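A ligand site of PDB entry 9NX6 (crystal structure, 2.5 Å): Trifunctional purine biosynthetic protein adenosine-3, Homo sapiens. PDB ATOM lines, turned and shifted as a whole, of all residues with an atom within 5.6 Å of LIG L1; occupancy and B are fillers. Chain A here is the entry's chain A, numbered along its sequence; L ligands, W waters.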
ATOM      1  N   ASN A  37     -33.718 -18.394  10.256  1.00  0.00           N
ATOM      2  CA  ASN A  37     -33.314 -19.681  10.811  1.00  0.00           C
ATOM      3  C   ASN A  37     -34.479 -20.644  10.912  1.00  0.00           C
ATOM      4  O   ASN A  37     -34.260 -21.817  11.273  1.00  0.00           O
ATOM      5  CB  ASN A  37     -32.671 -19.507  12.181  1.00  0.00           C
ATOM      6  CG  ASN A  37     -33.647 -19.065  13.255  1.00  0.00           C
ATOM      7  OD1 ASN A  37     -34.519 -18.235  13.014  1.00  0.00           O
ATOM      8  ND2 ASN A  37     -33.486 -19.611  14.460  1.00  0.00           N
ATOM      9  N   HIS A  59     -30.803 -24.281  12.346  1.00  0.00           N
ATOM     10  CA  HIS A  59     -29.877 -24.492  13.462  1.00  0.00           C
ATOM     11  C   HIS A  59     -30.072 -25.863  14.078  1.00  0.00           C
ATOM     12  O   HIS A  59     -29.774 -26.072  15.252  1.00  0.00           O
ATOM     13  CB  HIS A  59     -30.022 -23.406  14.522  1.00  0.00           C
ATOM     14  CG  HIS A  59     -31.402 -23.289  15.104  1.00  0.00           C
ATOM     15  ND1 HIS A  59     -32.361 -22.460  14.579  1.00  0.00           N
ATOM     16  CD2 HIS A  59     -31.961 -23.883  16.183  1.00  0.00           C
ATOM     17  CE1 HIS A  59     -33.466 -22.552  15.297  1.00  0.00           C
ATOM     18  NE2 HIS A  59     -33.252 -23.415  16.283  1.00  0.00           N
ATOM     19  N   ARG A  65     -23.153 -23.626  17.957  1.00  0.00           N
ATOM     20  CA  ARG A  65     -23.497 -22.252  17.663  1.00  0.00           C
ATOM     21  C   ARG A  65     -22.460 -21.641  16.719  1.00  0.00           C
ATOM     22  O   ARG A  65     -22.805 -20.882  15.811  1.00  0.00           O
ATOM     23  CB  ARG A  65     -23.607 -21.454  18.956  1.00  0.00           C
ATOM     24  CG  ARG A  65     -24.761 -20.497  18.968  1.00  0.00           C
ATOM     25  CD  ARG A  65     -24.759 -19.678  20.241  1.00  0.00           C
ATOM     26  NE  ARG A  65     -25.495 -20.351  21.320  1.00  0.00           N
ATOM     27  CZ  ARG A  65     -26.822 -20.490  21.366  1.00  0.00           C
ATOM     28  NH1 ARG A  65     -27.596 -19.997  20.413  1.00  0.00           N
ATOM     29  NH2 ARG A  65     -27.374 -21.118  22.397  1.00  0.00           N
ATOM     30  N   LEU A  86     -30.653  -7.483  12.723  1.00  0.00           N
ATOM     31  CA  LEU A  86     -31.472  -8.517  13.357  1.00  0.00           C
ATOM     32  C   LEU A  86     -32.889  -7.969  13.553  1.00  0.00           C
ATOM     33  O   LEU A  86     -33.098  -7.039  14.349  1.00  0.00           O
ATOM     34  CB  LEU A  86     -30.855  -8.955  14.691  1.00  0.00           C
ATOM     35  CG  LEU A  86     -29.352  -9.269  14.755  1.00  0.00           C
ATOM     36  CD1 LEU A  86     -28.982  -9.841  16.115  1.00  0.00           C
ATOM     37  CD2 LEU A  86     -28.931 -10.240  13.665  1.00  0.00           C
ATOM     38  N   PHE A  89     -34.809 -11.809  14.938  1.00  0.00           N
ATOM     39  CA  PHE A  89     -33.983 -12.997  14.958  1.00  0.00           C
ATOM     40  C   PHE A  89     -33.967 -13.576  16.367  1.00  0.00           C
ATOM     41  O   PHE A  89     -33.476 -12.933  17.292  1.00  0.00           O
ATOM     42  CB  PHE A  89     -32.569 -12.636  14.506  1.00  0.00           C
ATOM     43  CG  PHE A  89     -31.726 -13.803  14.149  1.00  0.00           C
ATOM     44  CD1 PHE A  89     -32.102 -14.664  13.144  1.00  0.00           C
ATOM     45  CD2 PHE A  89     -30.545 -14.056  14.849  1.00  0.00           C
ATOM     46  CE1 PHE A  89     -31.325 -15.760  12.823  1.00  0.00           C
ATOM     47  CE2 PHE A  89     -29.764 -15.160  14.529  1.00  0.00           C
ATOM     48  CZ  PHE A  89     -30.147 -16.015  13.514  1.00  0.00           C
ATOM     49  N   MET A  90     -34.495 -14.772  16.539  1.00  0.00           N
ATOM     50  CA  MET A  90     -34.592 -15.345  17.886  1.00  0.00           C
ATOM     51  C   MET A  90     -33.507 -16.394  18.135  1.00  0.00           C
ATOM     52  O   MET A  90     -33.769 -17.539  18.511  1.00  0.00           O
ATOM     53  CB  MET A  90     -35.975 -15.947  18.097  1.00  0.00           C
ATOM     54  CG  MET A  90     -37.066 -14.942  18.033  1.00  0.00           C
ATOM     55  SD  MET A  90     -36.811 -13.829  19.413  1.00  0.00           S
ATOM     56  CE  MET A  90     -38.088 -12.599  19.138  1.00  0.00           C
ATOM     57  N   ARG A  91     -32.265 -16.012  17.883  1.00  0.00           N
ATOM     58  CA  ARG A  91     -31.178 -16.906  18.222  1.00  0.00           C
ATOM     59  C   ARG A  91     -29.972 -16.070  18.624  1.00  0.00           C
ATOM     60  O   ARG A  91     -29.707 -15.020  18.044  1.00  0.00           O
ATOM     61  CB  ARG A  91     -30.889 -17.828  17.043  1.00  0.00           C
ATOM     62  CG  ARG A  91     -29.941 -18.901  17.416  1.00  0.00           C
ATOM     63  CD  ARG A  91     -30.167 -20.162  16.624  1.00  0.00           C
ATOM     64  NE  ARG A  91     -29.204 -21.194  16.994  1.00  0.00           N
ATOM     65  CZ  ARG A  91     -27.882 -21.047  16.947  1.00  0.00           C
ATOM     66  NH1 ARG A  91     -27.335 -19.894  16.553  1.00  0.00           N
ATOM     67  NH2 ARG A  91     -27.091 -22.055  17.300  1.00  0.00           N
ATOM     68  N   ILE A  92     -29.256 -16.531  19.642  1.00  0.00           N
ATOM     69  CA  ILE A  92     -28.156 -15.767  20.215  1.00  0.00           C
ATOM     70  C   ILE A  92     -26.877 -16.096  19.470  1.00  0.00           C
ATOM     71  O   ILE A  92     -26.566 -17.263  19.228  1.00  0.00           O
ATOM     72  CB  ILE A  92     -28.008 -16.048  21.703  1.00  0.00           C
ATOM     73  CG1 ILE A  92     -29.112 -15.337  22.471  1.00  0.00           C
ATOM     74  CG2 ILE A  92     -26.640 -15.619  22.176  1.00  0.00           C
ATOM     75  CD1 ILE A  92     -29.360 -15.920  23.814  1.00  0.00           C
ATOM     76  N   LEU A  93     -26.129 -15.050  19.125  1.00  0.00           N
ATOM     77  CA  LEU A  93     -25.010 -15.193  18.212  1.00  0.00           C
ATOM     78  C   LEU A  93     -23.719 -15.418  18.978  1.00  0.00           C
ATOM     79  O   LEU A  93     -23.517 -14.884  20.076  1.00  0.00           O
ATOM     80  CB  LEU A  93     -24.886 -13.948  17.326  1.00  0.00           C
ATOM     81  CG  LEU A  93     -26.023 -13.835  16.301  1.00  0.00           C
ATOM     82  CD1 LEU A  93     -26.428 -12.410  16.057  1.00  0.00           C
ATOM     83  CD2 LEU A  93     -25.623 -14.498  15.002  1.00  0.00           C
ATOM     84  N   SER A  94     -22.850 -16.231  18.407  1.00  0.00           N
ATOM     85  CA  SER A  94     -21.611 -16.570  19.068  1.00  0.00           C
ATOM     86  C   SER A  94     -20.698 -15.345  19.187  1.00  0.00           C
ATOM     87  O   SER A  94     -20.796 -14.380  18.441  1.00  0.00           O
ATOM     88  CB  SER A  94     -20.903 -17.693  18.311  1.00  0.00           C
ATOM     89  OG  SER A  94     -20.410 -17.202  17.075  1.00  0.00           O
ATOM     90  N   VAL A  98     -20.046 -12.173  16.699  1.00  0.00           N
ATOM     91  CA  VAL A  98     -20.334 -10.800  17.109  1.00  0.00           C
ATOM     92  C   VAL A  98     -19.094  -9.936  16.987  1.00  0.00           C
ATOM     93  O   VAL A  98     -19.157  -8.780  16.560  1.00  0.00           O
ATOM     94  CB  VAL A  98     -20.903 -10.774  18.533  1.00  0.00           C
ATOM     95  CG1 VAL A  98     -21.095  -9.359  18.989  1.00  0.00           C
ATOM     96  CG2 VAL A  98     -22.211 -11.542  18.599  1.00  0.00           C
ATOM     97  N   ASN A 107     -29.683  -4.443  16.224  1.00  0.00           N
ATOM     98  CA  ASN A 107     -30.778  -5.243  16.747  1.00  0.00           C
ATOM     99  C   ASN A 107     -31.900  -4.334  17.192  1.00  0.00           C
ATOM    100  O   ASN A 107     -31.652  -3.252  17.730  1.00  0.00           O
ATOM    101  CB  ASN A 107     -30.311  -6.089  17.896  1.00  0.00           C
ATOM    102  CG  ASN A 107     -31.414  -6.922  18.474  1.00  0.00           C
ATOM    103  OD1 ASN A 107     -32.076  -7.667  17.757  1.00  0.00           O
ATOM    104  ND2 ASN A 107     -31.617  -6.822  19.785  1.00  0.00           N
ATOM    105  N   GLY A 118     -33.596  -9.278  27.541  1.00  0.00           N
ATOM    106  CA  GLY A 118     -34.056 -10.642  27.441  1.00  0.00           C
ATOM    107  C   GLY A 118     -35.238 -10.782  26.504  1.00  0.00           C
ATOM    108  O   GLY A 118     -35.640  -9.843  25.797  1.00  0.00           O
ATOM    109  N   SER A 119     -35.795 -11.986  26.493  1.00  0.00           N
ATOM    110  CA  SER A 119     -36.658 -12.360  25.383  1.00  0.00           C
ATOM    111  C   SER A 119     -38.127 -12.050  25.611  1.00  0.00           C
ATOM    112  O   SER A 119     -38.872 -11.914  24.639  1.00  0.00           O
ATOM    113  CB  SER A 119     -36.491 -13.853  25.084  1.00  0.00           C
ATOM    114  OG  SER A 119     -36.635 -14.599  26.273  1.00  0.00           O
ATOM    115  N   HIS A 138     -29.910  -0.900  18.763  1.00  0.00           N
ATOM    116  CA  HIS A 138     -28.597  -0.870  19.362  1.00  0.00           C
ATOM    117  C   HIS A 138     -27.684  -1.738  18.532  1.00  0.00           C
ATOM    118  O   HIS A 138     -28.135  -2.636  17.808  1.00  0.00           O
ATOM    119  CB  HIS A 138     -28.624  -1.365  20.819  1.00  0.00           C
ATOM    120  CG  HIS A 138     -28.955  -2.823  20.971  1.00  0.00           C
ATOM    121  ND1 HIS A 138     -28.004  -3.783  21.197  1.00  0.00           N
ATOM    122  CD2 HIS A 138     -30.146  -3.484  20.930  1.00  0.00           C
ATOM    123  CE1 HIS A 138     -28.572  -4.973  21.283  1.00  0.00           C
ATOM    124  NE2 HIS A 138     -29.875  -4.814  21.130  1.00  0.00           N
ATOM    125  N   PHE A 139     -26.401  -1.442  18.612  1.00  0.00           N
ATOM    126  CA  PHE A 139     -25.397  -2.332  18.050  1.00  0.00           C
ATOM    127  C   PHE A 139     -25.316  -3.613  18.879  1.00  0.00           C
ATOM    128  O   PHE A 139     -25.460  -3.591  20.105  1.00  0.00           O
ATOM    129  CB  PHE A 139     -24.037  -1.635  18.028  1.00  0.00           C
ATOM    130  CG  PHE A 139     -23.882  -0.616  16.940  1.00  0.00           C
ATOM    131  CD1 PHE A 139     -23.794  -1.012  15.620  1.00  0.00           C
ATOM    132  CD2 PHE A 139     -23.789   0.726  17.237  1.00  0.00           C
ATOM    133  CE1 PHE A 139     -23.639  -0.077  14.607  1.00  0.00           C
ATOM    134  CE2 PHE A 139     -23.647   1.666  16.227  1.00  0.00           C
ATOM    135  CZ  PHE A 139     -23.564   1.269  14.919  1.00  0.00           C
ATOM    136  N   VAL A 140     -25.075  -4.739  18.218  1.00  0.00           N
ATOM    137  CA  VAL A 140     -24.946  -5.994  18.939  1.00  0.00           C
ATOM    138  C   VAL A 140     -23.531  -6.107  19.510  1.00  0.00           C
ATOM    139  O   VAL A 140     -22.543  -6.109  18.776  1.00  0.00           O
ATOM    140  CB  VAL A 140     -25.270  -7.181  18.031  1.00  0.00           C
ATOM    141  CG1 VAL A 140     -25.027  -8.477  18.780  1.00  0.00           C
ATOM    142  CG2 VAL A 140     -26.714  -7.076  17.548  1.00  0.00           C
ATOM    143  N   ALA A 141     -23.445  -6.186  20.827  1.00  0.00           N
ATOM    144  CA  ALA A 141     -22.228  -6.531  21.539  1.00  0.00           C
ATOM    145  C   ALA A 141     -22.366  -7.959  22.087  1.00  0.00           C
ATOM    146  O   ALA A 141     -23.406  -8.609  21.941  1.00  0.00           O
ATOM    147  CB  ALA A 141     -21.971  -5.519  22.652  1.00  0.00           C
ATOM    148  N   GLU A 142     -21.301  -8.480  22.696  1.00  0.00           N
ATOM    149  CA  GLU A 142     -21.366  -9.867  23.156  1.00  0.00           C
ATOM    150  C   GLU A 142     -22.429 -10.042  24.237  1.00  0.00           C
ATOM    151  O   GLU A 142     -23.268 -10.956  24.158  1.00  0.00           O
ATOM    152  CB  GLU A 142     -19.995 -10.336  23.623  1.00  0.00           C
ATOM    153  CG  GLU A 142     -19.205 -10.945  22.488  1.00  0.00           C
ATOM    154  CD  GLU A 142     -17.861 -11.521  22.915  1.00  0.00           C
ATOM    155  OE1 GLU A 142     -16.807 -11.055  22.400  1.00  0.00           O
ATOM    156  OE2 GLU A 142     -17.859 -12.436  23.765  1.00  0.00           O
ATOM    157  N   ASP A 143     -22.444  -9.176  25.246  1.00  0.00           N
ATOM    158  CA  ASP A 143     -23.487  -9.221  26.268  1.00  0.00           C
ATOM    159  C   ASP A 143     -24.830  -8.818  25.657  1.00  0.00           C
ATOM    160  O   ASP A 143     -24.966  -7.720  25.106  1.00  0.00           O
ATOM    161  CB  ASP A 143     -23.132  -8.301  27.426  1.00  0.00           C
ATOM    162  CG  ASP A 143     -21.912  -8.788  28.183  1.00  0.00           C
ATOM    163  OD1 ASP A 143     -21.954  -9.923  28.692  1.00  0.00           O
ATOM    164  OD2 ASP A 143     -20.909  -8.040  28.240  1.00  0.00           O
ATOM    165  N   VAL A 144     -25.822  -9.702  25.780  1.00  0.00           N
ATOM    166  CA  VAL A 144     -27.072  -9.557  25.021  1.00  0.00           C
ATOM    167  C   VAL A 144     -27.810  -8.285  25.459  1.00  0.00           C
ATOM    168  O   VAL A 144     -27.828  -7.933  26.649  1.00  0.00           O
ATOM    169  CB  VAL A 144     -27.945 -10.816  25.177  1.00  0.00           C
ATOM    170  CG1 VAL A 144     -29.285 -10.655  24.475  1.00  0.00           C
ATOM    171  CG2 VAL A 144     -27.210 -12.032  24.630  1.00  0.00           C
ATOM    172  N   ASP A 145     -28.429  -7.602  24.495  1.00  0.00           N
ATOM    173  CA  ASP A 145     -29.110  -6.320  24.718  1.00  0.00           C
ATOM    174  C   ASP A 145     -28.263  -5.360  25.549  1.00  0.00           C
ATOM    175  O   ASP A 145     -28.753  -4.717  26.483  1.00  0.00           O
ATOM    176  CB  ASP A 145     -30.484  -6.522  25.355  1.00  0.00           C
ATOM    177  CG  ASP A 145     -31.297  -7.609  24.685  1.00  0.00           C
ATOM    178  OD1 ASP A 145     -31.309  -7.656  23.429  1.00  0.00           O
ATOM    179  OD2 ASP A 145     -31.904  -8.426  25.413  1.00  0.00           O
ATOM    180  N   ALA A 146     -26.972  -5.264  25.212  1.00  0.00           N
ATOM    181  CA  ALA A 146     -26.063  -4.444  26.004  1.00  0.00           C
ATOM    182  C   ALA A 146     -25.100  -3.627  25.141  1.00  0.00           C
ATOM    183  O   ALA A 146     -24.205  -2.981  25.688  1.00  0.00           O
ATOM    184  CB  ALA A 146     -25.269  -5.328  26.994  1.00  0.00           C
HETATM  185  C1  LIG L   1     -32.959 -14.905  22.023  1.00  0.00           C
HETATM  186  C2  LIG L   1     -32.782 -15.812  23.096  1.00  0.00           C
HETATM  187  C3  LIG L   1     -33.116 -13.346  23.812  1.00  0.00           C
HETATM  188  C4  LIG L   1     -33.134 -13.554  22.424  1.00  0.00           C
HETATM  189  C5  LIG L   1     -33.186 -19.958  20.529  1.00  0.00           C
HETATM  190  C6  LIG L   1     -34.664 -20.090  20.890  1.00  0.00           C
HETATM  191  C7  LIG L   1     -32.546 -17.318  23.026  1.00  0.00           C
HETATM  192  C8  LIG L   1     -35.401 -20.881  19.811  1.00  0.00           C
HETATM  193  N1  LIG L   1     -24.257 -12.086  21.420  1.00  0.00           N
HETATM  194  C9  LIG L   1     -32.308 -19.407  21.645  1.00  0.00           C
HETATM  195  C10 LIG L   1     -25.516 -11.466  21.128  1.00  0.00           C
HETATM  196  C11 LIG L   1     -26.941  -9.661  21.351  1.00  0.00           C
HETATM  197  C12 LIG L   1     -29.226  -9.853  20.140  1.00  0.00           C
HETATM  198  C13 LIG L   1     -29.942 -10.746  19.327  1.00  0.00           C
HETATM  199  C14 LIG L   1     -27.901 -10.328  20.548  1.00  0.00           C
HETATM  200  C15 LIG L   1     -27.576 -11.589  20.045  1.00  0.00           C
HETATM  201  C16 LIG L   1     -30.840 -19.621  21.242  1.00  0.00           C
HETATM  202  C17 LIG L   1     -31.329 -10.565  18.731  1.00  0.00           C
HETATM  203  C18 LIG L   1     -32.401 -10.779  19.804  1.00  0.00           C
HETATM  204  C19 LIG L   1     -32.106 -11.993  20.678  1.00  0.00           C
HETATM  205  C20 LIG L   1     -33.361 -12.442  21.403  1.00  0.00           C
HETATM  206  F1  LIG L   1     -32.965 -15.290  20.719  1.00  0.00           F
HETATM  207  N2  LIG L   1     -26.382 -12.127  20.359  1.00  0.00           N
HETATM  208  N3  LIG L   1     -25.773 -10.249  21.632  1.00  0.00           N
HETATM  209  N4  LIG L   1     -32.550 -17.993  21.739  1.00  0.00           N
HETATM  210  O1  LIG L   1     -27.199  -8.585  21.782  1.00  0.00           O
HETATM  211  O2  LIG L   1     -32.353 -17.933  24.011  1.00  0.00           O
HETATM  212  O3  LIG L   1     -36.411 -21.579  20.121  1.00  0.00           O
HETATM  213  O4  LIG L   1     -35.004 -20.841  18.608  1.00  0.00           O
HETATM  214  O5  LIG L   1     -30.369 -20.786  21.262  1.00  0.00           O
HETATM  215  O6  LIG L   1     -30.123 -18.649  20.882  1.00  0.00           O
HETATM  216  S1  LIG L   1     -28.930 -12.074  19.107  1.00  0.00           S
HETATM  217  S2  LIG L   1     -32.864 -14.880  24.487  1.00  0.00           S
HETATM  218  C1  LG2 L   2     -40.176  -7.382  17.328  1.00  0.00           C
HETATM  219  O1  LG2 L   2     -41.341  -6.946  18.011  1.00  0.00           O
HETATM  220  C2  LG2 L   2     -38.949  -7.202  18.219  1.00  0.00           C
HETATM  221  O2  LG2 L   2     -39.062  -6.122  19.153  1.00  0.00           O
HETATM  222  C3  LG2 L   2     -38.868  -8.566  18.875  1.00  0.00           C
HETATM  223  O3  LG2 L   2     -39.509  -9.505  17.996  1.00  0.00           O
HETATM  224  C4  LG2 L   2     -40.391  -8.875  17.053  1.00  0.00           C
HETATM  225  C5  LG2 L   2     -40.185  -9.321  15.621  1.00  0.00           C
HETATM  226  O4  LG2 L   2     -41.397  -8.946  14.954  1.00  0.00           O
HETATM  227  N1  LG2 L   2     -37.564  -9.104  19.197  1.00  0.00           N
HETATM  228  C6  LG2 L   2     -37.360  -9.567  20.454  1.00  0.00           C
HETATM  229  O5  LG2 L   2     -38.270  -9.729  21.300  1.00  0.00           O
HETATM  230  C7  LG2 L   2     -35.893  -9.845  20.747  1.00  0.00           C
HETATM  231  N2  LG2 L   2     -35.631 -10.211  22.134  1.00  0.00           N
HETATM  232  P1  LG2 L   2     -41.450  -8.986  13.364  1.00  0.00           P
HETATM  233  O6  LG2 L   2     -42.892  -8.724  13.003  1.00  0.00           O
HETATM  234  O7  LG2 L   2     -40.464  -7.881  12.972  1.00  0.00           O
HETATM  235  O8  LG2 L   2     -41.007 -10.396  13.054  1.00  0.00           O
HETATM  236  O   HOH W   1     -33.309  -8.320  21.845  1.00  0.00           O
HETATM  237  O   HOH W   2     -25.591  -6.519  22.497  1.00  0.00           O
HETATM  238  O   HOH W   3     -32.574 -10.640  23.607  1.00  0.00           O
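The backbone NH of Ile 92 lies within hydrogen-bond range of an oxygen (O6) of LIG L1 (2.6 Å). N4 of LIG L1 lies close to O of Met 90. The backbone carbonyl oxygen (O) of Ala 141 sits at hydrogen-bond distance from a nitrogen (N3) of LIG L1 (2.9 Å). NH1 of Arg 65 is in salt-bridge range of O6 of LIG L1. The backbone carbonyl oxygen (O) of Glu 142 is in hydrogen-bond range of a nitrogen (N1) of LIG L1 (3.1 Å). N of Asp 145 lies within hydrogen-bond range of O1 of LIG L1. A nitrogen (N2) of LIG L1 is in hydrogen-bond range of the backbone NH (N) of Leu 93, 3.2 Å away. O of Leu 93 is in hydrogen-bond range of N1 of LIG L1 (3.2 Å).
NH1 of Arg 65 lies within hydrogen-bond range of O of Ile 92, at 3.2 Å. The side-chain carboxylate of Asp 145 sits at hydrogen-bond distance from the backbone NH of Gly 118 (2.8 Å). O of His 138 lies within hydrogen-bond range of N of Asn 107 (2.9 Å). A ring nitrogen (ND1) of His 59 sits close to the side-chain amide nitrogen (ND2) of Asn 37 (3.1 Å).
The backbone NH (N) of Arg 91 sits close to a fluorine (F1) of LIG L1 (3.0 Å). Residues that only touch LIG L1: His 59, Leu 86, Phe 89, Val 98, Asn 107, Ser 119, His 138, Val 140 and Val 144. Hydrophobic or aromatic side chains within 4 Å of LIG L1: Leu 86, Ile 92, Leu 93, Val 98, His 138, Val 140 and Val 144. 17 residues have an atom within 4 Å of LIG L1: His 59, Arg 65, Leu 86, Phe 89, Met 90, Arg 91, Ile 92, Leu 93, Val 98, Asn 107, Ser 119, His 138, Val 140, Ala 141, Glu 142, Val 144 and Asp 145. The nearest printed residue that does not touch LIG L1 is Asp 143 (4.1 Å).
Water W2 lies within hydrogen-bond range of O1 of LIG L1 (2.7 Å), N of Ala 141 (2.7 Å), O of Asp 143 (2.9 Å) and N of Ala 146 (3.3 Å). Water W3 lies within hydrogen-bond range of OD2 of Asp 145 (2.9 Å) and N2 of LG2 L2 (3.4 Å). Water W1 lies within hydrogen-bond range of the side-chain carboxylate (OD1) of Asp 145 (2.6 Å), a nitrogen (N2) of LG2 L2 (3.0 Å) and the side-chain amide nitrogen (ND2) of Asn 107 (3.1 Å).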
